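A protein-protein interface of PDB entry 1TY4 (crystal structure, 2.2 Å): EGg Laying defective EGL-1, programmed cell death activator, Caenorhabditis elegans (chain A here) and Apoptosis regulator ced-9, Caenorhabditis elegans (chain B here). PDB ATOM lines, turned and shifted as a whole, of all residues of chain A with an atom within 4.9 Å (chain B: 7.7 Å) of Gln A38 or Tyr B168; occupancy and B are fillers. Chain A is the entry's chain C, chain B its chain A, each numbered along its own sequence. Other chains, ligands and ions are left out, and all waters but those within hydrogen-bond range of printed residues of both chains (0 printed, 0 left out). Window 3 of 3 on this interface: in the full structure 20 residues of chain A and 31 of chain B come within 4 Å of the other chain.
No residue of chain B comes within 4 Å of Ala A37.
Gln A38 touches three residues of chain B.
Ser A41 touches none of the printed residues of chain B.
Printed residues of chain B within 4 Å of Tyr A42: Leu B160 (3.9 Å), Gln B163 (3.4 Å), Met B164 (3.6 Å) and Asp B167 (2.5 Å).
Of the printed residues of chain A, Leu B160 touches Met A39, Met A40 and Tyr A42.
The nearest printed residue of chain A that does not touch Tyr B168 is Tyr A42 (5.1 Å).
Ile B55 touches Phe A35.
Phe A35 touches Phe B56 (CD1 to CD1, 3.5 Å).
CE of Lys B59 touches CE1 of Phe A35, 3.9 Å away.
CZ of Phe A35 touches CE of Met B164, 3.6 Å away.
NZ of Lys B59 touches OE1 of Gln A38 (3.7 Å).
CE of Met B164 touches CD of Gln A38, 3.2 Å away.
Met B164 touches Met A39.
SD of Met A40 touches CD1 of Leu B160, 3.8 Å away.
Leu B160 touches Tyr A42 (CD2 to C, 3.9 Å).
Tyr A42 touches Gln B163.
OD2 of Asp B167 lies within hydrogen-bond range of OH of Tyr A42, 2.5 Å away.
The side-chain hydroxyl (OH) of Tyr B168 sits at hydrogen-bond distance from the side-chain amide nitrogen (NE2) of Gln A38, 3.1 Å away.
Of the 9 printed residues of chain A, 5 touch a printed residue of chain B.
Printed residues of chain B that touch a printed residue of chain A: Ile B55, Phe B56, Lys B59, Leu B160, Gln B163, Met B164, Asp B167 and Tyr B168.
Hydrophobic or aromatic side chains of chain B within 4 Å of the printed part of chain A: Ile B55, Phe B56, Leu B160, Met B164 and Tyr B168.
Among the printed residues, no Asp or Glu carboxylate lies within 4 Å of a Lys or Arg side-chain nitrogen of the other chain.
The side-chain hydroxyl of Tyr B168 is in hydrogen-bond range of the side-chain amino group of Lys B59, 2.5 Å away.
O of Gln A38 lies within hydrogen-bond range of OG of Ser A41 (2.6 Å).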
ATOM      1  N   ASP A  34       2.732 -24.142  14.203  1.00  0.00           N
ATOM      2  CA  ASP A  34       2.200 -23.033  14.979  1.00  0.00           C
ATOM      3  C   ASP A  34       2.909 -23.015  16.334  1.00  0.00           C
ATOM      4  O   ASP A  34       3.262 -21.949  16.832  1.00  0.00           O
ATOM      5  CB  ASP A  34       0.687 -23.170  15.186  1.00  0.00           C
ATOM      6  CG  ASP A  34      -0.117 -22.858  13.927  1.00  0.00           C
ATOM      7  OD1 ASP A  34       0.478 -22.432  12.914  1.00  0.00           O
ATOM      8  OD2 ASP A  34      -1.355 -23.037  13.954  1.00  0.00           O
ATOM      9  N   PHE A  35       3.123 -24.187  16.932  1.00  0.00           N
ATOM     10  CA  PHE A  35       3.805 -24.249  18.229  1.00  0.00           C
ATOM     11  C   PHE A  35       5.251 -23.767  18.092  1.00  0.00           C
ATOM     12  O   PHE A  35       5.751 -23.030  18.942  1.00  0.00           O
ATOM     13  CB  PHE A  35       3.820 -25.677  18.777  1.00  0.00           C
ATOM     14  CG  PHE A  35       4.122 -25.760  20.250  1.00  0.00           C
ATOM     15  CD1 PHE A  35       3.095 -25.726  21.183  1.00  0.00           C
ATOM     16  CD2 PHE A  35       5.431 -25.873  20.703  1.00  0.00           C
ATOM     17  CE1 PHE A  35       3.364 -25.809  22.552  1.00  0.00           C
ATOM     18  CE2 PHE A  35       5.714 -25.955  22.066  1.00  0.00           C
ATOM     19  CZ  PHE A  35       4.678 -25.925  22.992  1.00  0.00           C
ATOM     20  N   ASP A  36       5.915 -24.199  17.021  1.00  0.00           N
ATOM     21  CA  ASP A  36       7.300 -23.825  16.764  1.00  0.00           C
ATOM     22  C   ASP A  36       7.422 -22.308  16.600  1.00  0.00           C
ATOM     23  O   ASP A  36       8.300 -21.677  17.192  1.00  0.00           O
ATOM     24  CB  ASP A  36       7.805 -24.526  15.504  1.00  0.00           C
ATOM     25  CG  ASP A  36       9.311 -24.405  15.332  1.00  0.00           C
ATOM     26  OD1 ASP A  36      10.052 -24.870  16.228  1.00  0.00           O
ATOM     27  OD2 ASP A  36       9.754 -23.851  14.301  1.00  0.00           O
ATOM     28  N   ALA A  37       6.533 -21.729  15.797  1.00  0.00           N
ATOM     29  CA  ALA A  37       6.538 -20.291  15.565  1.00  0.00           C
ATOM     30  C   ALA A  37       6.477 -19.540  16.895  1.00  0.00           C
ATOM     31  O   ALA A  37       7.259 -18.620  17.136  1.00  0.00           O
ATOM     32  CB  ALA A  37       5.356 -19.899  14.684  1.00  0.00           C
ATOM     33  N   GLN A  38       5.550 -19.939  17.760  1.00  0.00           N
ATOM     34  CA  GLN A  38       5.404 -19.295  19.059  1.00  0.00           C
ATOM     35  C   GLN A  38       6.657 -19.444  19.913  1.00  0.00           C
ATOM     36  O   GLN A  38       7.172 -18.468  20.456  1.00  0.00           O
ATOM     37  CB  GLN A  38       4.202 -19.876  19.808  1.00  0.00           C
ATOM     38  CG  GLN A  38       4.261 -19.678  21.313  1.00  0.00           C
ATOM     39  CD  GLN A  38       2.924 -19.907  21.998  1.00  0.00           C
ATOM     40  OE1 GLN A  38       2.148 -20.782  21.607  1.00  0.00           O
ATOM     41  NE2 GLN A  38       2.658 -19.128  23.040  1.00  0.00           N
ATOM     42  N   MET A  39       7.139 -20.675  20.026  1.00  0.00           N
ATOM     43  CA  MET A  39       8.325 -20.976  20.817  1.00  0.00           C
ATOM     44  C   MET A  39       9.545 -20.232  20.268  1.00  0.00           C
ATOM     45  O   MET A  39      10.391 -19.772  21.023  1.00  0.00           O
ATOM     46  CB  MET A  39       8.563 -22.493  20.801  1.00  0.00           C
ATOM     47  CG  MET A  39       9.645 -23.023  21.740  1.00  0.00           C
ATOM     48  SD  MET A  39       9.768 -24.987  21.629  1.00  0.00           S
ATOM     49  CE  MET A  39       9.568 -25.109  19.722  1.00  0.00           C
ATOM     50  N   MET A  40       9.615 -20.100  18.950  1.00  0.00           N
ATOM     51  CA  MET A  40      10.730 -19.424  18.302  1.00  0.00           C
ATOM     52  C   MET A  40      10.676 -17.896  18.455  1.00  0.00           C
ATOM     53  O   MET A  40      11.565 -17.189  17.977  1.00  0.00           O
ATOM     54  CB  MET A  40      10.758 -19.794  16.818  1.00  0.00           C
ATOM     55  CG  MET A  40      12.150 -19.992  16.232  1.00  0.00           C
ATOM     56  SD  MET A  40      13.154 -21.396  17.122  1.00  0.00           S
ATOM     57  CE  MET A  40      11.713 -22.631  17.457  1.00  0.00           C
ATOM     58  N   SER A  41       9.641 -17.391  19.122  1.00  0.00           N
ATOM     59  CA  SER A  41       9.498 -15.951  19.318  1.00  0.00           C
ATOM     60  C   SER A  41      10.195 -15.477  20.594  1.00  0.00           C
ATOM     61  O   SER A  41      10.163 -14.290  20.919  1.00  0.00           O
ATOM     62  CB  SER A  41       8.020 -15.555  19.370  1.00  0.00           C
ATOM     63  OG  SER A  41       7.446 -15.886  20.622  1.00  0.00           O
ATOM     64  N   TYR A  42      10.805 -16.404  21.328  1.00  0.00           N
ATOM     65  CA  TYR A  42      11.535 -16.041  22.539  1.00  0.00           C
ATOM     66  C   TYR A  42      12.986 -15.827  22.162  1.00  0.00           C
ATOM     67  O   TYR A  42      13.801 -15.391  22.970  1.00  0.00           O
ATOM     68  CB  TYR A  42      11.434 -17.133  23.591  1.00  0.00           C
ATOM     69  CG  TYR A  42      10.049 -17.264  24.149  1.00  0.00           C
ATOM     70  CD1 TYR A  42       9.138 -18.151  23.590  1.00  0.00           C
ATOM     71  CD2 TYR A  42       9.637 -16.478  25.220  1.00  0.00           C
ATOM     72  CE1 TYR A  42       7.849 -18.257  24.079  1.00  0.00           C
ATOM     73  CE2 TYR A  42       8.348 -16.572  25.720  1.00  0.00           C
ATOM     74  CZ  TYR A  42       7.457 -17.469  25.142  1.00  0.00           C
ATOM     75  OH  TYR A  42       6.178 -17.592  25.625  1.00  0.00           O
ATOM     76  N   VAL B  51       6.996 -31.015  29.922  1.00  0.00           N
ATOM     77  CA  VAL B  51       6.236 -29.773  30.016  1.00  0.00           C
ATOM     78  C   VAL B  51       5.731 -29.338  28.643  1.00  0.00           C
ATOM     79  O   VAL B  51       4.542 -29.068  28.471  1.00  0.00           O
ATOM     80  CB  VAL B  51       7.086 -28.633  30.627  1.00  0.00           C
ATOM     81  CG1 VAL B  51       6.257 -27.356  30.707  1.00  0.00           C
ATOM     82  CG2 VAL B  51       7.578 -29.035  32.019  1.00  0.00           C
ATOM     83  N   MET B  52       6.633 -29.272  27.669  1.00  0.00           N
ATOM     84  CA  MET B  52       6.258 -28.875  26.313  1.00  0.00           C
ATOM     85  C   MET B  52       5.152 -29.791  25.780  1.00  0.00           C
ATOM     86  O   MET B  52       4.179 -29.327  25.178  1.00  0.00           O
ATOM     87  CB  MET B  52       7.475 -28.935  25.383  1.00  0.00           C
ATOM     88  CG  MET B  52       8.557 -27.913  25.693  1.00  0.00           C
ATOM     89  SD  MET B  52       7.983 -26.051  25.460  1.00  0.00           S
ATOM     90  CE  MET B  52       7.107 -25.777  27.157  1.00  0.00           C
ATOM     91  N   ILE B  55       1.798 -28.984  27.439  1.00  0.00           N
ATOM     92  CA  ILE B  55       1.263 -27.732  26.906  1.00  0.00           C
ATOM     93  C   ILE B  55       0.688 -27.999  25.524  1.00  0.00           C
ATOM     94  O   ILE B  55      -0.415 -27.570  25.205  1.00  0.00           O
ATOM     95  CB  ILE B  55       2.361 -26.649  26.760  1.00  0.00           C
ATOM     96  CG1 ILE B  55       2.790 -26.140  28.140  1.00  0.00           C
ATOM     97  CG2 ILE B  55       1.855 -25.511  25.884  1.00  0.00           C
ATOM     98  CD1 ILE B  55       3.947 -25.151  28.089  1.00  0.00           C
ATOM     99  N   PHE B  56       1.446 -28.715  24.706  1.00  0.00           N
ATOM    100  CA  PHE B  56       1.004 -29.015  23.355  1.00  0.00           C
ATOM    101  C   PHE B  56      -0.333 -29.762  23.336  1.00  0.00           C
ATOM    102  O   PHE B  56      -1.244 -29.409  22.580  1.00  0.00           O
ATOM    103  CB  PHE B  56       2.067 -29.844  22.632  1.00  0.00           C
ATOM    104  CG  PHE B  56       1.845 -29.949  21.162  1.00  0.00           C
ATOM    105  CD1 PHE B  56       2.425 -29.031  20.293  1.00  0.00           C
ATOM    106  CD2 PHE B  56       1.026 -30.946  20.639  1.00  0.00           C
ATOM    107  CE1 PHE B  56       2.190 -29.099  18.925  1.00  0.00           C
ATOM    108  CE2 PHE B  56       0.783 -31.025  19.272  1.00  0.00           C
ATOM    109  CZ  PHE B  56       1.363 -30.102  18.410  1.00  0.00           C
ATOM    110  N   LYS B  58      -2.716 -29.961  25.689  1.00  0.00           N
ATOM    111  CA  LYS B  58      -3.833 -29.179  26.202  1.00  0.00           C
ATOM    112  C   LYS B  58      -4.412 -28.267  25.126  1.00  0.00           C
ATOM    113  O   LYS B  58      -5.621 -28.057  25.070  1.00  0.00           O
ATOM    114  CB  LYS B  58      -3.397 -28.367  27.425  1.00  0.00           C
ATOM    115  CG  LYS B  58      -3.076 -29.236  28.630  1.00  0.00           C
ATOM    116  CD  LYS B  58      -2.603 -28.415  29.817  1.00  0.00           C
ATOM    117  CE  LYS B  58      -2.340 -29.297  31.030  1.00  0.00           C
ATOM    118  NZ  LYS B  58      -1.787 -28.521  32.182  1.00  0.00           N
ATOM    119  N   LYS B  59      -3.546 -27.746  24.263  1.00  0.00           N
ATOM    120  CA  LYS B  59      -3.976 -26.866  23.182  1.00  0.00           C
ATOM    121  C   LYS B  59      -4.834 -27.589  22.150  1.00  0.00           C
ATOM    122  O   LYS B  59      -5.767 -27.017  21.590  1.00  0.00           O
ATOM    123  CB  LYS B  59      -2.765 -26.288  22.440  1.00  0.00           C
ATOM    124  CG  LYS B  59      -1.902 -25.303  23.211  1.00  0.00           C
ATOM    125  CD  LYS B  59      -0.708 -24.884  22.356  1.00  0.00           C
ATOM    126  CE  LYS B  59       0.101 -23.769  23.006  1.00  0.00           C
ATOM    127  NZ  LYS B  59      -0.706 -22.523  23.175  1.00  0.00           N
ATOM    128  N   LEU B 160      14.662 -21.522  25.086  1.00  0.00           N
ATOM    129  CA  LEU B 160      13.351 -21.111  24.603  1.00  0.00           C
ATOM    130  C   LEU B 160      12.266 -21.777  25.450  1.00  0.00           C
ATOM    131  O   LEU B 160      11.327 -21.117  25.906  1.00  0.00           O
ATOM    132  CB  LEU B 160      13.189 -21.488  23.128  1.00  0.00           C
ATOM    133  CG  LEU B 160      14.281 -20.997  22.172  1.00  0.00           C
ATOM    134  CD1 LEU B 160      14.025 -21.535  20.774  1.00  0.00           C
ATOM    135  CD2 LEU B 160      14.313 -19.469  22.154  1.00  0.00           C
ATOM    136  N   GLY B 161      12.417 -23.080  25.681  1.00  0.00           N
ATOM    137  CA  GLY B 161      11.449 -23.823  26.471  1.00  0.00           C
ATOM    138  C   GLY B 161      11.284 -23.290  27.882  1.00  0.00           C
ATOM    139  O   GLY B 161      10.184 -23.298  28.437  1.00  0.00           O
ATOM    140  N   LYS B 162      12.379 -22.832  28.477  1.00  0.00           N
ATOM    141  CA  LYS B 162      12.306 -22.285  29.823  1.00  0.00           C
ATOM    142  C   LYS B 162      11.377 -21.073  29.791  1.00  0.00           C
ATOM    143  O   LYS B 162      10.424 -20.981  30.566  1.00  0.00           O
ATOM    144  CB  LYS B 162      13.692 -21.876  30.301  1.00  0.00           C
ATOM    145  N   GLN B 163      11.655 -20.154  28.872  1.00  0.00           N
ATOM    146  CA  GLN B 163      10.858 -18.940  28.724  1.00  0.00           C
ATOM    147  C   GLN B 163       9.374 -19.223  28.476  1.00  0.00           C
ATOM    148  O   GLN B 163       8.502 -18.618  29.104  1.00  0.00           O
ATOM    149  CB  GLN B 163      11.417 -18.090  27.583  1.00  0.00           C
ATOM    150  CG  GLN B 163      12.717 -17.376  27.915  1.00  0.00           C
ATOM    151  CD  GLN B 163      13.334 -16.703  26.705  1.00  0.00           C
ATOM    152  OE1 GLN B 163      13.971 -17.351  25.875  1.00  0.00           O
ATOM    153  NE2 GLN B 163      13.133 -15.395  26.591  1.00  0.00           N
ATOM    154  N   MET B 164       9.089 -20.144  27.563  1.00  0.00           N
ATOM    155  CA  MET B 164       7.705 -20.481  27.246  1.00  0.00           C
ATOM    156  C   MET B 164       6.993 -21.103  28.444  1.00  0.00           C
ATOM    157  O   MET B 164       5.817 -20.827  28.693  1.00  0.00           O
ATOM    158  CB  MET B 164       7.659 -21.433  26.050  1.00  0.00           C
ATOM    159  CG  MET B 164       6.255 -21.844  25.633  1.00  0.00           C
ATOM    160  SD  MET B 164       6.210 -22.585  23.846  1.00  0.00           S
ATOM    161  CE  MET B 164       4.322 -22.416  23.487  1.00  0.00           C
ATOM    162  N   LYS B 165       7.715 -21.939  29.184  1.00  0.00           N
ATOM    163  CA  LYS B 165       7.163 -22.599  30.362  1.00  0.00           C
ATOM    164  C   LYS B 165       6.669 -21.585  31.392  1.00  0.00           C
ATOM    165  O   LYS B 165       5.579 -21.725  31.949  1.00  0.00           O
ATOM    166  CB  LYS B 165       8.229 -23.492  30.999  1.00  0.00           C
ATOM    167  CG  LYS B 165       7.841 -24.072  32.350  1.00  0.00           C
ATOM    168  CD  LYS B 165       8.982 -24.879  32.935  1.00  0.00           C
ATOM    169  CE  LYS B 165       8.632 -25.399  34.317  1.00  0.00           C
ATOM    170  NZ  LYS B 165       9.767 -26.146  34.929  1.00  0.00           N
ATOM    171  N   GLU B 166       7.478 -20.563  31.641  1.00  0.00           N
ATOM    172  CA  GLU B 166       7.120 -19.539  32.612  1.00  0.00           C
ATOM    173  C   GLU B 166       5.831 -18.811  32.238  1.00  0.00           C
ATOM    174  O   GLU B 166       4.957 -18.608  33.082  1.00  0.00           O
ATOM    175  CB  GLU B 166       8.268 -18.546  32.760  1.00  0.00           C
ATOM    176  CG  GLU B 166       9.613 -19.221  32.926  1.00  0.00           C
ATOM    177  CD  GLU B 166      10.556 -18.437  33.809  1.00  0.00           C
ATOM    178  OE1 GLU B 166      10.593 -17.196  33.681  1.00  0.00           O
ATOM    179  OE2 GLU B 166      11.267 -19.065  34.625  1.00  0.00           O
ATOM    180  N   ASP B 167       5.707 -18.425  30.973  1.00  0.00           N
ATOM    181  CA  ASP B 167       4.511 -17.732  30.514  1.00  0.00           C
ATOM    182  C   ASP B 167       3.256 -18.550  30.775  1.00  0.00           C
ATOM    183  O   ASP B 167       2.215 -18.005  31.139  1.00  0.00           O
ATOM    184  CB  ASP B 167       4.608 -17.420  29.021  1.00  0.00           C
ATOM    185  CG  ASP B 167       5.576 -16.300  28.727  1.00  0.00           C
ATOM    186  OD1 ASP B 167       5.420 -15.212  29.318  1.00  0.00           O
ATOM    187  OD2 ASP B 167       6.490 -16.504  27.906  1.00  0.00           O
ATOM    188  N   TYR B 168       3.351 -19.860  30.583  1.00  0.00           N
ATOM    189  CA  TYR B 168       2.202 -20.722  30.803  1.00  0.00           C
ATOM    190  C   TYR B 168       1.950 -21.011  32.275  1.00  0.00           C
ATOM    191  O   TYR B 168       0.846 -21.406  32.652  1.00  0.00           O
ATOM    192  CB  TYR B 168       2.357 -22.027  30.022  1.00  0.00           C
ATOM    193  CG  TYR B 168       2.010 -21.865  28.563  1.00  0.00           C
ATOM    194  CD1 TYR B 168       2.900 -21.261  27.674  1.00  0.00           C
ATOM    195  CD2 TYR B 168       0.758 -22.247  28.083  1.00  0.00           C
ATOM    196  CE1 TYR B 168       2.548 -21.037  26.345  1.00  0.00           C
ATOM    197  CE2 TYR B 168       0.395 -22.026  26.762  1.00  0.00           C
ATOM    198  CZ  TYR B 168       1.293 -21.422  25.900  1.00  0.00           C
ATOM    199  OH  TYR B 168       0.926 -21.194  24.598  1.00  0.00           O
ATOM    200  N   GLU B 169       2.967 -20.809  33.106  1.00  0.00           N
ATOM    201  CA  GLU B 169       2.818 -21.042  34.537  1.00  0.00           C
ATOM    202  C   GLU B 169       2.367 -19.760  35.232  1.00  0.00           C
ATOM    203  O   GLU B 169       2.298 -19.693  36.461  1.00  0.00           O
ATOM    204  CB  GLU B 169       4.134 -21.549  35.138  1.00  0.00           C
ATOM    205  CG  GLU B 169       4.558 -22.910  34.597  1.00  0.00           C
ATOM    206  CD  GLU B 169       5.618 -23.586  35.447  1.00  0.00           C
ATOM    207  OE1 GLU B 169       6.736 -23.039  35.565  1.00  0.00           O
ATOM    208  OE2 GLU B 169       5.330 -24.670  36.000  1.00  0.00           O
ATOM    209  N   ARG B 170       2.056 -18.749  34.420  1.00  0.00           N
ATOM    210  CA  ARG B 170       1.588 -17.449  34.898  1.00  0.00           C
ATOM    211  C   ARG B 170       2.651 -16.651  35.645  1.00  0.00           C
ATOM    212  O   ARG B 170       2.450 -16.380  36.849  1.00  0.00           O
ATOM    213  CB  ARG B 170       0.361 -17.631  35.791  1.00  0.00           C
ATOM    214  CG  ARG B 170      -0.808 -18.303  35.102  1.00  0.00           C
ATOM    215  CD  ARG B 170      -1.239 -19.528  35.878  1.00  0.00           C
ATOM    216  NE  ARG B 170      -2.585 -19.956  35.521  1.00  0.00           N
ATOM    217  CZ  ARG B 170      -3.319 -20.783  36.258  1.00  0.00           C
ATOM    218  NH1 ARG B 170      -2.831 -21.271  37.391  1.00  0.00           N
ATOM    219  NH2 ARG B 170      -4.543 -21.112  35.870  1.00  0.00           N
ATOM    220  OXT ARG B 170       3.670 -16.298  35.013  1.00  0.00           O
